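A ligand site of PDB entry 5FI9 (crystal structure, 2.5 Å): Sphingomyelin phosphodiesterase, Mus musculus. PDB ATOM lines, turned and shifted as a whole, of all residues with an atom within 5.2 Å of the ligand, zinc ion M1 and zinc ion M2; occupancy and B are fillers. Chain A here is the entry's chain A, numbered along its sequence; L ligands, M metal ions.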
ATOM      1  N   ASP A 131      17.267   9.678 -23.680  1.00  0.00           N
ATOM      2  CA  ASP A 131      17.793   8.498 -22.998  1.00  0.00           C
ATOM      3  C   ASP A 131      16.926   8.115 -21.808  1.00  0.00           C
ATOM      4  O   ASP A 131      17.394   7.972 -20.679  1.00  0.00           O
ATOM      5  CB  ASP A 131      19.246   8.740 -22.564  1.00  0.00           C
ATOM      6  CG  ASP A 131      20.145   9.140 -23.724  1.00  0.00           C
ATOM      7  OD1 ASP A 131      20.757   8.247 -24.339  1.00  0.00           O
ATOM      8  OD2 ASP A 131      20.224  10.358 -24.020  1.00  0.00           O
ATOM      9  N   HIS A 133      15.232   5.208 -21.645  1.00  0.00           N
ATOM     10  CA  HIS A 133      15.617   3.812 -21.429  1.00  0.00           C
ATOM     11  C   HIS A 133      14.687   3.131 -20.419  1.00  0.00           C
ATOM     12  O   HIS A 133      15.071   2.801 -19.296  1.00  0.00           O
ATOM     13  CB  HIS A 133      17.079   3.723 -20.967  1.00  0.00           C
ATOM     14  CG  HIS A 133      18.073   4.135 -22.015  1.00  0.00           C
ATOM     15  ND1 HIS A 133      18.340   3.353 -23.113  1.00  0.00           N
ATOM     16  CD2 HIS A 133      18.862   5.222 -22.124  1.00  0.00           C
ATOM     17  CE1 HIS A 133      19.259   3.952 -23.859  1.00  0.00           C
ATOM     18  NE2 HIS A 133      19.595   5.090 -23.280  1.00  0.00           N
ATOM     19  N   ASP A 203      16.440   6.878 -27.810  1.00  0.00           N
ATOM     20  CA  ASP A 203      16.884   5.895 -26.819  1.00  0.00           C
ATOM     21  C   ASP A 203      15.774   5.623 -25.796  1.00  0.00           C
ATOM     22  O   ASP A 203      15.848   5.992 -24.626  1.00  0.00           O
ATOM     23  CB  ASP A 203      18.190   6.341 -26.148  1.00  0.00           C
ATOM     24  CG  ASP A 203      19.422   5.799 -26.837  1.00  0.00           C
ATOM     25  OD1 ASP A 203      20.532   5.898 -26.262  1.00  0.00           O
ATOM     26  OD2 ASP A 203      19.286   5.258 -27.962  1.00  0.00           O
ATOM     27  N   HIS A 207      18.610  -1.433 -22.160  1.00  0.00           N
ATOM     28  CA  HIS A 207      19.797  -2.063 -22.723  1.00  0.00           C
ATOM     29  C   HIS A 207      19.730  -3.583 -22.692  1.00  0.00           C
ATOM     30  O   HIS A 207      20.783  -4.238 -22.727  1.00  0.00           O
ATOM     31  CB  HIS A 207      21.045  -1.575 -21.987  1.00  0.00           C
ATOM     32  CG  HIS A 207      21.204  -0.085 -21.998  1.00  0.00           C
ATOM     33  ND1 HIS A 207      20.384   0.764 -21.279  1.00  0.00           N
ATOM     34  CD2 HIS A 207      22.102   0.712 -22.627  1.00  0.00           C
ATOM     35  CE1 HIS A 207      20.763   2.014 -21.476  1.00  0.00           C
ATOM     36  NE2 HIS A 207      21.805   2.007 -22.297  1.00  0.00           N
ATOM     37  N   ASN A 243      19.765   5.172 -31.085  1.00  0.00           N
ATOM     38  CA  ASN A 243      20.437   3.975 -31.559  1.00  0.00           C
ATOM     39  C   ASN A 243      19.914   2.690 -30.938  1.00  0.00           C
ATOM     40  O   ASN A 243      20.202   1.610 -31.460  1.00  0.00           O
ATOM     41  CB  ASN A 243      21.950   4.081 -31.307  1.00  0.00           C
ATOM     42  CG  ASN A 243      22.284   4.305 -29.842  1.00  0.00           C
ATOM     43  OD1 ASN A 243      21.690   5.146 -29.178  1.00  0.00           O
ATOM     44  ND2 ASN A 243      23.241   3.532 -29.337  1.00  0.00           N
ATOM     45  N   HIS A 244      19.140   2.777 -29.857  1.00  0.00           N
ATOM     46  CA  HIS A 244      18.542   1.596 -29.234  1.00  0.00           C
ATOM     47  C   HIS A 244      17.149   1.292 -29.749  1.00  0.00           C
ATOM     48  O   HIS A 244      16.573   0.254 -29.387  1.00  0.00           O
ATOM     49  CB  HIS A 244      18.494   1.768 -27.715  1.00  0.00           C
ATOM     50  CG  HIS A 244      19.808   1.583 -27.031  1.00  0.00           C
ATOM     51  ND1 HIS A 244      20.200   0.383 -26.485  1.00  0.00           N
ATOM     52  CD2 HIS A 244      20.826   2.447 -26.804  1.00  0.00           C
ATOM     53  CE1 HIS A 244      21.405   0.508 -25.949  1.00  0.00           C
ATOM     54  NE2 HIS A 244      21.803   1.758 -26.122  1.00  0.00           N
ATOM     55  N   HIS A 350      20.510  12.340 -31.850  1.00  0.00           N
ATOM     56  CA  HIS A 350      20.820  11.537 -30.677  1.00  0.00           C
ATOM     57  C   HIS A 350      22.324  11.512 -30.418  1.00  0.00           C
ATOM     58  O   HIS A 350      22.802  12.097 -29.445  1.00  0.00           O
ATOM     59  CB  HIS A 350      20.293  10.112 -30.834  1.00  0.00           C
ATOM     60  CG  HIS A 350      20.591   9.251 -29.656  1.00  0.00           C
ATOM     61  ND1 HIS A 350      20.063   9.495 -28.404  1.00  0.00           N
ATOM     62  CD2 HIS A 350      21.372   8.157 -29.527  1.00  0.00           C
ATOM     63  CE1 HIS A 350      20.504   8.588 -27.552  1.00  0.00           C
ATOM     64  NE2 HIS A 350      21.303   7.759 -28.206  1.00  0.00           N
ATOM     65  N   HIS A 382      22.777  10.918 -25.727  1.00  0.00           N
ATOM     66  CA  HIS A 382      23.569   9.711 -25.994  1.00  0.00           C
ATOM     67  C   HIS A 382      24.699   9.514 -24.981  1.00  0.00           C
ATOM     68  O   HIS A 382      25.026   8.371 -24.638  1.00  0.00           O
ATOM     69  CB  HIS A 382      24.139   9.764 -27.414  1.00  0.00           C
ATOM     70  CG  HIS A 382      24.775   8.481 -27.855  1.00  0.00           C
ATOM     71  ND1 HIS A 382      24.073   7.289 -27.925  1.00  0.00           N
ATOM     72  CD2 HIS A 382      26.033   8.205 -28.275  1.00  0.00           C
ATOM     73  CE1 HIS A 382      24.887   6.343 -28.353  1.00  0.00           C
ATOM     74  NE2 HIS A 382      26.079   6.868 -28.570  1.00  0.00           N
ATOM     75  N   THR A 383      25.296  10.603 -24.493  1.00  0.00           N
ATOM     76  CA  THR A 383      26.379  10.473 -23.526  1.00  0.00           C
ATOM     77  C   THR A 383      25.875  10.213 -22.109  1.00  0.00           C
ATOM     78  O   THR A 383      26.631   9.698 -21.285  1.00  0.00           O
ATOM     79  CB  THR A 383      27.234  11.744 -23.515  1.00  0.00           C
ATOM     80  OG1 THR A 383      26.438  12.865 -23.118  1.00  0.00           O
ATOM     81  CG2 THR A 383      27.820  12.003 -24.891  1.00  0.00           C
ATOM     82  N   HIS A 384      24.620  10.574 -21.820  1.00  0.00           N
ATOM     83  CA  HIS A 384      23.976  10.401 -20.529  1.00  0.00           C
ATOM     84  C   HIS A 384      24.539  11.333 -19.462  1.00  0.00           C
ATOM     85  O   HIS A 384      24.119  11.240 -18.296  1.00  0.00           O
ATOM     86  CB  HIS A 384      24.055   8.952 -20.019  1.00  0.00           C
ATOM     87  CG  HIS A 384      23.330   7.964 -20.879  1.00  0.00           C
ATOM     88  ND1 HIS A 384      22.846   6.770 -20.396  1.00  0.00           N
ATOM     89  CD2 HIS A 384      22.992   8.001 -22.191  1.00  0.00           C
ATOM     90  CE1 HIS A 384      22.249   6.103 -21.369  1.00  0.00           C
ATOM     91  NE2 HIS A 384      22.326   6.833 -22.474  1.00  0.00           N
ATOM     92  N   VAL A 385      25.460  12.231 -19.803  1.00  0.00           N
ATOM     93  CA  VAL A 385      26.043  13.177 -18.864  1.00  0.00           C
ATOM     94  C   VAL A 385      25.865  14.586 -19.427  1.00  0.00           C
ATOM     95  O   VAL A 385      25.520  14.770 -20.595  1.00  0.00           O
ATOM     96  CB  VAL A 385      27.525  12.879 -18.577  1.00  0.00           C
ATOM     97  CG1 VAL A 385      27.659  11.660 -17.678  1.00  0.00           C
ATOM     98  CG2 VAL A 385      28.297  12.668 -19.873  1.00  0.00           C
ATOM     99  N   PHE A 413      21.528   4.574 -15.819  1.00  0.00           N
ATOM    100  CA  PHE A 413      22.627   3.969 -16.568  1.00  0.00           C
ATOM    101  C   PHE A 413      23.715   4.998 -16.919  1.00  0.00           C
ATOM    102  O   PHE A 413      23.461   5.847 -17.773  1.00  0.00           O
ATOM    103  CB  PHE A 413      22.054   3.336 -17.843  1.00  0.00           C
ATOM    104  CG  PHE A 413      22.896   2.224 -18.406  1.00  0.00           C
ATOM    105  CD1 PHE A 413      22.753   0.932 -17.938  1.00  0.00           C
ATOM    106  CD2 PHE A 413      23.806   2.470 -19.414  1.00  0.00           C
ATOM    107  CE1 PHE A 413      23.516  -0.095 -18.462  1.00  0.00           C
ATOM    108  CE2 PHE A 413      24.570   1.457 -19.942  1.00  0.00           C
ATOM    109  CZ  PHE A 413      24.425   0.167 -19.464  1.00  0.00           C
ATOM    110  N   ILE A 414      24.903   4.968 -16.307  1.00  0.00           N
ATOM    111  CA  ILE A 414      25.305   4.059 -15.217  1.00  0.00           C
ATOM    112  C   ILE A 414      25.714   4.885 -14.009  1.00  0.00           C
ATOM    113  O   ILE A 414      26.467   5.848 -14.138  1.00  0.00           O
ATOM    114  CB  ILE A 414      26.474   3.143 -15.653  1.00  0.00           C
ATOM    115  CG1 ILE A 414      26.055   2.237 -16.806  1.00  0.00           C
ATOM    116  CG2 ILE A 414      26.971   2.297 -14.477  1.00  0.00           C
ATOM    117  CD1 ILE A 414      27.207   1.848 -17.719  1.00  0.00           C
ATOM    118  N   LEU A 416      24.210   7.038 -12.147  1.00  0.00           N
ATOM    119  CA  LEU A 416      23.838   8.434 -12.287  1.00  0.00           C
ATOM    120  C   LEU A 416      22.468   8.660 -11.665  1.00  0.00           C
ATOM    121  O   LEU A 416      21.714   7.721 -11.408  1.00  0.00           O
ATOM    122  CB  LEU A 416      23.802   8.865 -13.767  1.00  0.00           C
ATOM    123  CG  LEU A 416      25.126   8.890 -14.512  1.00  0.00           C
ATOM    124  CD1 LEU A 416      24.887   8.949 -16.019  1.00  0.00           C
ATOM    125  CD2 LEU A 416      25.973  10.065 -14.062  1.00  0.00           C
ATOM    126  N   TYR A 499      28.421  17.304 -14.205  1.00  0.00           N
ATOM    127  CA  TYR A 499      28.649  16.328 -15.261  1.00  0.00           C
ATOM    128  C   TYR A 499      27.866  15.048 -15.008  1.00  0.00           C
ATOM    129  O   TYR A 499      27.190  14.531 -15.899  1.00  0.00           O
ATOM    130  CB  TYR A 499      30.150  16.042 -15.354  1.00  0.00           C
ATOM    131  CG  TYR A 499      30.614  15.232 -16.547  1.00  0.00           C
ATOM    132  CD1 TYR A 499      31.050  15.849 -17.712  1.00  0.00           C
ATOM    133  CD2 TYR A 499      30.646  13.845 -16.492  1.00  0.00           C
ATOM    134  CE1 TYR A 499      31.499  15.117 -18.794  1.00  0.00           C
ATOM    135  CE2 TYR A 499      31.082  13.096 -17.581  1.00  0.00           C
ATOM    136  CZ  TYR A 499      31.514  13.735 -18.722  1.00  0.00           C
ATOM    137  OH  TYR A 499      31.948  13.006 -19.796  1.00  0.00           O
ATOM    138  N   HIS A 500      27.938  14.536 -13.773  1.00  0.00           N
ATOM    139  CA  HIS A 500      27.269  13.293 -13.402  1.00  0.00           C
ATOM    140  C   HIS A 500      25.933  13.527 -12.706  1.00  0.00           C
ATOM    141  O   HIS A 500      25.466  12.663 -11.964  1.00  0.00           O
ATOM    142  CB  HIS A 500      28.186  12.461 -12.506  1.00  0.00           C
ATOM    143  CG  HIS A 500      29.557  12.246 -13.068  1.00  0.00           C
ATOM    144  ND1 HIS A 500      29.920  11.095 -13.728  1.00  0.00           N
ATOM    145  CD2 HIS A 500      30.652  13.048 -13.075  1.00  0.00           C
ATOM    146  CE1 HIS A 500      31.175  11.182 -14.121  1.00  0.00           C
ATOM    147  NE2 HIS A 500      31.645  12.364 -13.739  1.00  0.00           N
HETATM  148  N1  LIG L   1      26.075   5.531 -25.201  1.00  0.00           N
HETATM  149  C1  LIG L   1      25.207   4.546 -24.659  1.00  0.00           C
HETATM  150  C2  LIG L   1      25.244   4.574 -23.149  1.00  0.00           C
HETATM  151  C3  LIG L   1      26.430   5.318 -22.593  1.00  0.00           C
HETATM  152  C4  LIG L   1      26.594   5.073 -21.111  1.00  0.00           C
HETATM  153  C5  LIG L   1      27.266   6.240 -20.417  1.00  0.00           C
HETATM  154  C6  LIG L   1      27.489   5.978 -18.945  1.00  0.00           C
HETATM  155  C7  LIG L   1      27.903   7.225 -18.201  1.00  0.00           C
HETATM  156  C8  LIG L   1      29.299   7.106 -17.642  1.00  0.00           C
HETATM  157  C9  LIG L   1      29.677   8.307 -16.804  1.00  0.00           C
HETATM  158  C10 LIG L   1      29.566   8.008 -15.328  1.00  0.00           C
HETATM  159  P1  LIG L   1      23.508   4.820 -25.237  1.00  0.00           P
HETATM  160  O1  LIG L   1      22.554   4.002 -24.409  1.00  0.00           O
HETATM  161  O2  LIG L   1      23.394   4.397 -26.679  1.00  0.00           O
HETATM  162  O3  LIG L   1      23.175   6.286 -25.100  1.00  0.00           O
HETATM  163  P2  LIG L   1      25.742   2.900 -25.223  1.00  0.00           P
HETATM  164  O4  LIG L   1      26.164   2.981 -26.670  1.00  0.00           O
HETATM  165  O5  LIG L   1      24.589   1.926 -25.076  1.00  0.00           O
HETATM  166  O6  LIG L   1      26.900   2.431 -24.377  1.00  0.00           O
HETATM  167 ZN    ZN M   1      21.076   6.243 -24.084  1.00  0.00          ZN
HETATM  168 ZN    ZN M   2      22.329   6.153 -27.451  1.00  0.00          ZN
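Zinc ion M2 is bound by a ring nitrogen (NE2) of His 350 (2.0 Å), the side-chain amide oxygen (OD1) of Asn 243 (2.1 Å), a ring nitrogen (ND1) of His 382 (2.1 Å), the side-chain carboxylate (OD1) of Asp 203 (2.2 Å), an oxygen (O2) of the ligand (2.2 Å) and an oxygen (O3) of the ligand (2.5 Å).
Four residues have an atom within 4 Å of zinc ion M1: Asp 131, His 133, Asp 203 and His 384. The nearest printed residue that does not touch zinc ion M1 is His 350 (4.2 Å).
A ring nitrogen (NE2) of His 244 lies within hydrogen-bond range of an oxygen (O1) of the ligand, 2.9 Å away. A ring nitrogen (NE2) of His 207 sits at hydrogen-bond distance from an oxygen (O1) of the ligand (3.0 Å). The backbone carbonyl oxygen (O) of His 382 is in hydrogen-bond range of a nitrogen (N1) of the ligand, 3.1 Å away.
O of Thr 383 touches C5 of the ligand (3.6 Å). Ile 414 touches the ligand. His 500 touches the ligand (ND1 to C10, 3.5 Å). Hydrophobic or aromatic side chains that line the ligand: His 133, His 207, His 244, His 382, His 384 and His 500. Within 4 Å of the ligand: Asp 131, His 133, Asp 203, His 207, Asn 243, His 244, His 350, His 382, Thr 383, His 384, Ile 414 and His 500.
O of Val 385 sits at hydrogen-bond distance from OG1 of Thr 383 (3.3 Å). The backbone NH (N) of His 382 is in hydrogen-bond range of the side-chain carboxylate (OD2) of Asp 131 (3.1 Å). The side-chain carboxylate (OD2) of Asp 203 sits at hydrogen-bond distance from the backbone NH (N) of His 244 (3.1 Å). A ring nitrogen (ND1) of His 384 is in hydrogen-bond range of the backbone carbonyl oxygen (O) of Phe 413, 2.8 Å away.
Within 4 Å of zinc ion M2: Asp 203, Asn 243, His 350 and His 382.
Zinc ion M1 is bound by NE2 of His 133 (2.0 Å), OD1 of Asp 131 (2.0 Å), NE2 of His 384 (2.1 Å), OD1 of Asp 203 (2.3 Å) and O3 of the ligand (2.3 Å). Slightly farther from zinc ion M1 lies an oxygen (O1) of the ligand (2.7 Å).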
